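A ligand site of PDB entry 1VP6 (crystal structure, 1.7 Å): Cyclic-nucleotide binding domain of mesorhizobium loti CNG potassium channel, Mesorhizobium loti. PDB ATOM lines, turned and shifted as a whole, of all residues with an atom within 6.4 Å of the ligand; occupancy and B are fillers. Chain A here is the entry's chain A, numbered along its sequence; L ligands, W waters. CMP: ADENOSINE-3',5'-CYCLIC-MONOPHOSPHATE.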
ATOM      1  N   CYS A  46     -19.508  18.674  22.364  1.00  0.00           N
ATOM      2  CA  CYS A  46     -18.344  17.793  22.405  1.00  0.00           C
ATOM      3  C   CYS A  46     -17.396  18.296  21.333  1.00  0.00           C
ATOM      4  O   CYS A  46     -17.829  18.697  20.241  1.00  0.00           O
ATOM      5  CB  CYS A  46     -18.728  16.313  22.199  1.00  0.00           C
ATOM      6  SG  CYS A  46     -19.392  15.824  20.597  1.00  0.00           S
ATOM      7  N   GLY A  52     -14.538  10.705  24.822  1.00  0.00           N
ATOM      8  CA  GLY A  52     -15.971  10.751  25.023  1.00  0.00           C
ATOM      9  C   GLY A  52     -16.436   9.594  25.886  1.00  0.00           C
ATOM     10  O   GLY A  52     -16.107   8.446  25.621  1.00  0.00           O
ATOM     11  N   ARG A  54     -19.906   9.516  26.983  1.00  0.00           N
ATOM     12  CA  ARG A  54     -21.356   9.622  27.020  1.00  0.00           C
ATOM     13  C   ARG A  54     -21.880  10.014  25.633  1.00  0.00           C
ATOM     14  O   ARG A  54     -21.108  10.445  24.779  1.00  0.00           O
ATOM     15  CB  ARG A  54     -21.784  10.689  28.029  1.00  0.00           C
ATOM     16  CG  ARG A  54     -21.364  12.111  27.660  1.00  0.00           C
ATOM     17  CD  ARG A  54     -21.442  13.051  28.860  1.00  0.00           C
ATOM     18  NE  ARG A  54     -20.492  12.650  29.897  1.00  0.00           N
ATOM     19  CZ  ARG A  54     -20.316  13.309  31.043  1.00  0.00           C
ATOM     20  NH1 ARG A  54     -21.014  14.409  31.294  1.00  0.00           N
ATOM     21  NH2 ARG A  54     -19.422  12.884  31.925  1.00  0.00           N
ATOM     22  N   VAL A  65     -23.249  19.179  13.526  1.00  0.00           N
ATOM     23  CA  VAL A  65     -22.038  18.357  13.547  1.00  0.00           C
ATOM     24  C   VAL A  65     -21.083  19.001  12.544  1.00  0.00           C
ATOM     25  O   VAL A  65     -21.410  19.122  11.360  1.00  0.00           O
ATOM     26  CB  VAL A  65     -22.351  16.901  13.119  1.00  0.00           C
ATOM     27  CG1 VAL A  65     -21.092  16.036  13.234  1.00  0.00           C
ATOM     28  CG2 VAL A  65     -23.460  16.338  13.982  1.00  0.00           C
ATOM     29  N   THR A  67     -18.794  18.425  10.391  1.00  0.00           N
ATOM     30  CA  THR A  67     -18.118  17.572   9.432  1.00  0.00           C
ATOM     31  C   THR A  67     -17.834  18.517   8.252  1.00  0.00           C
ATOM     32  O   THR A  67     -18.411  19.592   8.179  1.00  0.00           O
ATOM     33  CB  THR A  67     -19.030  16.421   8.973  1.00  0.00           C
ATOM     34  OG1 THR A  67     -20.364  16.907   8.800  1.00  0.00           O
ATOM     35  CG2 THR A  67     -19.034  15.302   9.999  1.00  0.00           C
ATOM     36  N   VAL A  71     -23.653  18.676   9.313  1.00  0.00           N
ATOM     37  CA  VAL A  71     -24.894  17.917   9.381  1.00  0.00           C
ATOM     38  C   VAL A  71     -25.739  18.407  10.563  1.00  0.00           C
ATOM     39  O   VAL A  71     -25.250  18.486  11.693  1.00  0.00           O
ATOM     40  CB  VAL A  71     -24.605  16.417   9.575  1.00  0.00           C
ATOM     41  CG1 VAL A  71     -25.913  15.637   9.738  1.00  0.00           C
ATOM     42  CG2 VAL A  71     -23.811  15.882   8.373  1.00  0.00           C
ATOM     43  N   LEU A  73     -28.826  18.009  13.234  1.00  0.00           N
ATOM     44  CA  LEU A  73     -29.574  16.943  13.892  1.00  0.00           C
ATOM     45  C   LEU A  73     -30.614  17.597  14.789  1.00  0.00           C
ATOM     46  O   LEU A  73     -30.280  18.305  15.735  1.00  0.00           O
ATOM     47  CB  LEU A  73     -28.631  16.048  14.711  1.00  0.00           C
ATOM     48  CG  LEU A  73     -27.545  15.308  13.917  1.00  0.00           C
ATOM     49  CD1 LEU A  73     -26.662  14.503  14.859  1.00  0.00           C
ATOM     50  CD2 LEU A  73     -28.205  14.389  12.898  1.00  0.00           C
ATOM     51  N   PHE A  78     -29.782  11.549  17.688  1.00  0.00           N
ATOM     52  CA  PHE A  78     -28.764  11.274  18.703  1.00  0.00           C
ATOM     53  C   PHE A  78     -27.379  11.432  18.116  1.00  0.00           C
ATOM     54  O   PHE A  78     -27.189  11.331  16.912  1.00  0.00           O
ATOM     55  CB  PHE A  78     -28.961   9.870  19.314  1.00  0.00           C
ATOM     56  CG  PHE A  78     -28.854   8.742  18.321  1.00  0.00           C
ATOM     57  CD1 PHE A  78     -27.609   8.339  17.830  1.00  0.00           C
ATOM     58  CD2 PHE A  78     -29.987   8.054  17.897  1.00  0.00           C
ATOM     59  CE1 PHE A  78     -27.503   7.280  16.939  1.00  0.00           C
ATOM     60  CE2 PHE A  78     -29.893   6.999  16.999  1.00  0.00           C
ATOM     61  CZ  PHE A  78     -28.645   6.602  16.519  1.00  0.00           C
ATOM     62  N   PHE A  79     -26.417  11.704  18.985  1.00  0.00           N
ATOM     63  CA  PHE A  79     -25.031  11.874  18.550  1.00  0.00           C
ATOM     64  C   PHE A  79     -24.104  11.565  19.707  1.00  0.00           C
ATOM     65  O   PHE A  79     -24.527  11.515  20.856  1.00  0.00           O
ATOM     66  CB  PHE A  79     -24.808  13.301  18.019  1.00  0.00           C
ATOM     67  CG  PHE A  79     -24.989  14.380  19.050  1.00  0.00           C
ATOM     68  CD1 PHE A  79     -23.910  14.813  19.824  1.00  0.00           C
ATOM     69  CD2 PHE A  79     -26.229  14.981  19.246  1.00  0.00           C
ATOM     70  CE1 PHE A  79     -24.062  15.828  20.767  1.00  0.00           C
ATOM     71  CE2 PHE A  79     -26.398  16.001  20.191  1.00  0.00           C
ATOM     72  CZ  PHE A  79     -25.311  16.424  20.959  1.00  0.00           C
ATOM     73  N   GLY A  80     -22.823  11.370  19.379  1.00  0.00           N
ATOM     74  CA  GLY A  80     -21.843  11.048  20.405  1.00  0.00           C
ATOM     75  C   GLY A  80     -21.721   9.556  20.621  1.00  0.00           C
ATOM     76  O   GLY A  80     -20.995   9.110  21.515  1.00  0.00           O
ATOM     77  N   GLU A  81     -22.438   8.772  19.822  1.00  0.00           N
ATOM     78  CA  GLU A  81     -22.404   7.327  19.941  1.00  0.00           C
ATOM     79  C   GLU A  81     -21.135   6.685  19.396  1.00  0.00           C
ATOM     80  O   GLU A  81     -20.729   5.615  19.850  1.00  0.00           O
ATOM     81  CB  GLU A  81     -23.622   6.703  19.245  1.00  0.00           C
ATOM     82  CG  GLU A  81     -23.581   6.647  17.711  1.00  0.00           C
ATOM     83  CD  GLU A  81     -23.662   8.009  17.043  1.00  0.00           C
ATOM     84  OE1 GLU A  81     -24.126   8.973  17.678  1.00  0.00           O
ATOM     85  OE2 GLU A  81     -23.264   8.119  15.867  1.00  0.00           O
ATOM     86  N   MET A  82     -20.481   7.344  18.452  1.00  0.00           N
ATOM     87  CA  MET A  82     -19.277   6.795  17.862  1.00  0.00           C
ATOM     88  C   MET A  82     -18.118   6.571  18.829  1.00  0.00           C
ATOM     89  O   MET A  82     -17.414   5.570  18.737  1.00  0.00           O
ATOM     90  CB  MET A  82     -18.824   7.658  16.677  1.00  0.00           C
ATOM     91  CG  MET A  82     -19.793   7.550  15.501  1.00  0.00           C
ATOM     92  SD  MET A  82     -19.509   8.736  14.201  1.00  0.00           S
ATOM     93  CE  MET A  82     -18.006   8.120  13.491  1.00  0.00           C
ATOM     94  N   ALA A  83     -17.918   7.491  19.771  1.00  0.00           N
ATOM     95  CA  ALA A  83     -16.832   7.327  20.731  1.00  0.00           C
ATOM     96  C   ALA A  83     -17.138   6.144  21.644  1.00  0.00           C
ATOM     97  O   ALA A  83     -16.239   5.431  22.072  1.00  0.00           O
ATOM     98  CB  ALA A  83     -16.656   8.600  21.564  1.00  0.00           C
ATOM     99  N   LEU A  84     -18.421   5.953  21.933  1.00  0.00           N
ATOM    100  CA  LEU A  84     -18.845   4.850  22.797  1.00  0.00           C
ATOM    101  C   LEU A  84     -18.755   3.505  22.097  1.00  0.00           C
ATOM    102  O   LEU A  84     -18.416   2.490  22.711  1.00  0.00           O
ATOM    103  CB  LEU A  84     -20.279   5.075  23.287  1.00  0.00           C
ATOM    104  CG  LEU A  84     -20.479   6.268  24.225  1.00  0.00           C
ATOM    105  CD1 LEU A  84     -21.939   6.329  24.665  1.00  0.00           C
ATOM    106  CD2 LEU A  84     -19.569   6.122  25.444  1.00  0.00           C
ATOM    107  N   GLU A  88     -12.839   5.356  20.347  1.00  0.00           N
ATOM    108  CA  GLU A  88     -11.995   6.426  19.812  1.00  0.00           C
ATOM    109  C   GLU A  88     -12.461   7.808  20.278  1.00  0.00           C
ATOM    110  O   GLU A  88     -13.555   7.950  20.804  1.00  0.00           O
ATOM    111  CB  GLU A  88     -12.009   6.366  18.295  1.00  0.00           C
ATOM    112  CG  GLU A  88     -11.326   5.143  17.710  1.00  0.00           C
ATOM    113  CD  GLU A  88     -11.544   5.006  16.220  1.00  0.00           C
ATOM    114  OE1 GLU A  88     -11.508   6.035  15.512  1.00  0.00           O
ATOM    115  OE2 GLU A  88     -11.736   3.867  15.749  1.00  0.00           O
ATOM    116  N   PRO A  89     -11.609   8.841  20.095  1.00  0.00           N
ATOM    117  CA  PRO A  89     -11.963  10.208  20.499  1.00  0.00           C
ATOM    118  C   PRO A  89     -13.102  10.725  19.611  1.00  0.00           C
ATOM    119  O   PRO A  89     -13.381  10.137  18.566  1.00  0.00           O
ATOM    120  CB  PRO A  89     -10.664  10.981  20.251  1.00  0.00           C
ATOM    121  CG  PRO A  89      -9.601   9.927  20.399  1.00  0.00           C
ATOM    122  CD  PRO A  89     -10.204   8.760  19.663  1.00  0.00           C
ATOM    123  N   ARG A  90     -13.743  11.811  20.038  1.00  0.00           N
ATOM    124  CA  ARG A  90     -14.829  12.396  19.248  1.00  0.00           C
ATOM    125  C   ARG A  90     -14.370  12.589  17.808  1.00  0.00           C
ATOM    126  O   ARG A  90     -13.289  13.111  17.558  1.00  0.00           O
ATOM    127  CB  ARG A  90     -15.254  13.745  19.837  1.00  0.00           C
ATOM    128  CG  ARG A  90     -15.778  13.697  21.268  1.00  0.00           C
ATOM    129  CD  ARG A  90     -17.008  12.804  21.393  1.00  0.00           C
ATOM    130  NE  ARG A  90     -17.639  12.926  22.704  1.00  0.00           N
ATOM    131  CZ  ARG A  90     -18.635  12.168  23.134  1.00  0.00           C
ATOM    132  NH1 ARG A  90     -19.126  11.210  22.360  1.00  0.00           N
ATOM    133  NH2 ARG A  90     -19.146  12.347  24.350  1.00  0.00           N
ATOM    134  N   SER A  91     -15.201  12.170  16.857  1.00  0.00           N
ATOM    135  CA  SER A  91     -14.859  12.275  15.439  1.00  0.00           C
ATOM    136  C   SER A  91     -15.120  13.660  14.862  1.00  0.00           C
ATOM    137  O   SER A  91     -14.678  13.972  13.751  1.00  0.00           O
ATOM    138  CB  SER A  91     -15.646  11.231  14.631  1.00  0.00           C
ATOM    139  OG  SER A  91     -17.042  11.456  14.746  1.00  0.00           O
ATOM    140  N   ALA A  92     -15.845  14.485  15.600  1.00  0.00           N
ATOM    141  CA  ALA A  92     -16.149  15.827  15.124  1.00  0.00           C
ATOM    142  C   ALA A  92     -16.726  16.662  16.260  1.00  0.00           C
ATOM    143  O   ALA A  92     -17.180  16.121  17.271  1.00  0.00           O
ATOM    144  CB  ALA A  92     -17.157  15.761  13.975  1.00  0.00           C
ATOM    145  N   THR A  93     -16.677  17.975  16.086  1.00  0.00           N
ATOM    146  CA  THR A  93     -17.223  18.885  17.072  1.00  0.00           C
ATOM    147  C   THR A  93     -18.724  19.014  16.818  1.00  0.00           C
ATOM    148  O   THR A  93     -19.148  19.144  15.670  1.00  0.00           O
ATOM    149  CB  THR A  93     -16.580  20.282  16.952  1.00  0.00           C
ATOM    150  OG1 THR A  93     -15.212  20.214  17.362  1.00  0.00           O
ATOM    151  CG2 THR A  93     -17.324  21.302  17.825  1.00  0.00           C
ATOM    152  N   VAL A  94     -19.520  18.937  17.877  1.00  0.00           N
ATOM    153  CA  VAL A  94     -20.963  19.088  17.746  1.00  0.00           C
ATOM    154  C   VAL A  94     -21.315  20.275  18.609  1.00  0.00           C
ATOM    155  O   VAL A  94     -20.954  20.306  19.782  1.00  0.00           O
ATOM    156  CB  VAL A  94     -21.728  17.867  18.263  1.00  0.00           C
ATOM    157  CG1 VAL A  94     -23.235  18.095  18.079  1.00  0.00           C
ATOM    158  CG2 VAL A  94     -21.272  16.614  17.519  1.00  0.00           C
ATOM    159  N   GLU A 130     -22.497   3.987   9.505  1.00  0.00           N
ATOM    160  CA  GLU A 130     -22.864   4.818   8.362  1.00  0.00           C
ATOM    161  C   GLU A 130     -22.240   6.204   8.444  1.00  0.00           C
ATOM    162  O   GLU A 130     -21.794   6.755   7.438  1.00  0.00           O
ATOM    163  CB  GLU A 130     -24.390   4.944   8.282  1.00  0.00           C
ATOM    164  CG  GLU A 130     -24.887   5.839   7.168  1.00  0.00           C
ATOM    165  CD  GLU A 130     -26.384   5.783   7.001  1.00  0.00           C
ATOM    166  OE1 GLU A 130     -27.108   5.993   7.995  1.00  0.00           O
ATOM    167  OE2 GLU A 130     -26.858   5.522   5.871  1.00  0.00           O
ATOM    168  N   ARG A 131     -22.194   6.764   9.653  1.00  0.00           N
ATOM    169  CA  ARG A 131     -21.624   8.082   9.871  1.00  0.00           C
ATOM    170  C   ARG A 131     -20.108   8.102   9.787  1.00  0.00           C
ATOM    171  O   ARG A 131     -19.524   9.093   9.353  1.00  0.00           O
ATOM    172  CB  ARG A 131     -22.064   8.628  11.227  1.00  0.00           C
ATOM    173  CG  ARG A 131     -23.545   8.915  11.303  1.00  0.00           C
ATOM    174  CD  ARG A 131     -23.978   9.298  12.708  1.00  0.00           C
ATOM    175  NE  ARG A 131     -25.349   9.778  12.714  1.00  0.00           N
ATOM    176  CZ  ARG A 131     -26.011  10.142  13.805  1.00  0.00           C
ATOM    177  NH1 ARG A 131     -25.426  10.089  14.994  1.00  0.00           N
ATOM    178  NH2 ARG A 131     -27.258  10.581  13.703  1.00  0.00           N
ATOM    179  N   ARG A 132     -19.482   7.022  10.216  1.00  0.00           N
ATOM    180  CA  ARG A 132     -18.024   6.936  10.190  1.00  0.00           C
ATOM    181  C   ARG A 132     -17.540   6.937   8.746  1.00  0.00           C
ATOM    182  O   ARG A 132     -18.120   6.256   7.888  1.00  0.00           O
ATOM    183  CB  ARG A 132     -17.541   5.664  10.906  1.00  0.00           C
ATOM    184  CG  ARG A 132     -17.879   4.371  10.184  1.00  0.00           C
ATOM    185  CD  ARG A 132     -17.398   3.153  10.969  1.00  0.00           C
ATOM    186  NE  ARG A 132     -18.208   2.891  12.152  1.00  0.00           N
ATOM    187  CZ  ARG A 132     -18.017   1.861  12.978  1.00  0.00           C
ATOM    188  NH1 ARG A 132     -17.037   1.000  12.746  1.00  0.00           N
ATOM    189  NH2 ARG A 132     -18.813   1.695  14.021  1.00  0.00           N
ATOM    190  N   GLY A 133     -16.493   7.706   8.472  1.00  0.00           N
ATOM    191  CA  GLY A 133     -15.945   7.793   7.129  1.00  0.00           C
ATOM    192  C   GLY A 133     -16.959   8.311   6.125  1.00  0.00           C
ATOM    193  O   GLY A 133     -18.114   8.558   6.525  1.00  0.00           O
HETATM  194  P   CMP L   1     -18.610  10.941  18.275  1.00  0.00           P
HETATM  195  O1P CMP L   1     -17.410  10.684  17.446  1.00  0.00           O
HETATM  196  O2P CMP L   1     -18.482  10.219  19.575  1.00  0.00           O
HETATM  197  O5' CMP L   1     -18.719  12.434  18.488  1.00  0.00           O
HETATM  198  C5' CMP L   1     -18.916  13.338  17.368  1.00  0.00           C
HETATM  199  C4' CMP L   1     -20.358  12.964  17.019  1.00  0.00           C
HETATM  200  O4' CMP L   1     -21.001  13.654  15.958  1.00  0.00           O
HETATM  201  C3' CMP L   1     -20.430  11.493  16.638  1.00  0.00           C
HETATM  202  O3' CMP L   1     -19.966  10.576  17.632  1.00  0.00           O
HETATM  203  C2' CMP L   1     -21.739  11.356  15.905  1.00  0.00           C
HETATM  204  O2' CMP L   1     -22.803  11.156  16.742  1.00  0.00           O
HETATM  205  C1' CMP L   1     -21.661  12.724  15.070  1.00  0.00           C
HETATM  206  N9  CMP L   1     -21.487  12.536  13.510  1.00  0.00           N
HETATM  207  C8  CMP L   1     -20.186  12.300  12.993  1.00  0.00           C
HETATM  208  N7  CMP L   1     -20.109  12.151  11.687  1.00  0.00           N
HETATM  209  C5  CMP L   1     -21.431  12.316  11.317  1.00  0.00           C
HETATM  210  C6  CMP L   1     -22.146  12.297  10.068  1.00  0.00           C
HETATM  211  N6  CMP L   1     -21.569  12.091   8.885  1.00  0.00           N
HETATM  212  N1  CMP L   1     -23.511  12.511  10.156  1.00  0.00           N
HETATM  213  C2  CMP L   1     -24.235  12.725  11.290  1.00  0.00           C
HETATM  214  N3  CMP L   1     -23.598  12.753  12.503  1.00  0.00           N
HETATM  215  C4  CMP L   1     -22.278  12.544  12.365  1.00  0.00           C
HETATM  216  O   HOH W   1     -17.337  12.271  10.158  1.00  0.00           O
HETATM  217  O   HOH W   2     -15.553   8.553  17.662  1.00  0.00           O
HETATM  218  O   HOH W   3     -18.977  12.176   8.045  1.00  0.00           O
HETATM  219  O   HOH W   4     -23.254  12.752   6.554  1.00  0.00           O
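CG1 of Val 65 touches N9 of the ligand, at 3.5 Å.
CG2 of Thr 67 touches N7 of the ligand (3.7 Å).
CG1 of Val 71 touches C2 of the ligand, 3.7 Å away.
Phe 79 touches the ligand (CA to O2', 3.0 Å).
Ala 92 touches the ligand.
Val 94 touches the ligand.
Hydrophobic or aromatic side chains within 4 Å of the ligand: Val 65, Val 71, Phe 79, Met 82, Ala 83 and Val 94.
Along chain A the residues within 4 Å of the ligand span positions 65 to 131.
The backbone carbonyl oxygen (O) of Gly 80 sits at hydrogen-bond distance from the guanidinium group (NH1) of Arg 90 (2.9 Å).
The guanidinium group of Arg 131 lies within salt-bridge range of the side-chain carboxylate of Glu 81 (3.1 Å).
The side-chain sulfur of Met 82 sits close to the side-chain hydroxyl of Ser 91, 3.7 Å away.
The guanidinium group of Arg 90 is in hydrogen-bond range of the backbone carbonyl oxygen of Arg 54.
NH1 of Arg 131 is in hydrogen-bond range of O of Phe 78, at 2.9 Å.
The backbone carbonyl oxygen (O) of Cys 46 sits at hydrogen-bond distance from the backbone NH (N) of Val 94 (2.9 Å).
N of Val 65 is in hydrogen-bond range of O of Val 71 (2.8 Å).
An oxygen (O2') of the ligand lies within hydrogen-bond range of the backbone NH (N) of Gly 80 (2.6 Å).
The side-chain carboxylate (OE1) of Glu 81 is in hydrogen-bond range of an oxygen (O2') of the ligand, at 2.7 Å.
The backbone NH (N) of Ser 91 lies within hydrogen-bond range of an oxygen (O1P) of the ligand (2.7 Å).
OG of Ser 91 is in hydrogen-bond range of O1P of the ligand.
The backbone NH (N) of Ala 83 is in hydrogen-bond range of an oxygen (O2P) of the ligand, at 2.8 Å.
The guanidinium group of Arg 90 lies within salt-bridge range of an oxygen (O2P) of the ligand (3.0 Å).
N of Met 82 sits close to O3' of the ligand (3.4 Å).
NH1 of Arg 131 lies within hydrogen-bond range of O2' of the ligand (3.3 Å).
Water W3 lies within hydrogen-bond range of a nitrogen (N6) of the ligand and the backbone carbonyl oxygen of Arg 131.
Water W2 lies within hydrogen-bond range of an oxygen (O1P) of the ligand (2.8 Å), the backbone carbonyl oxygen of Pro 89 (2.8 Å) and the backbone NH of Ala 83 (3.3 Å).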
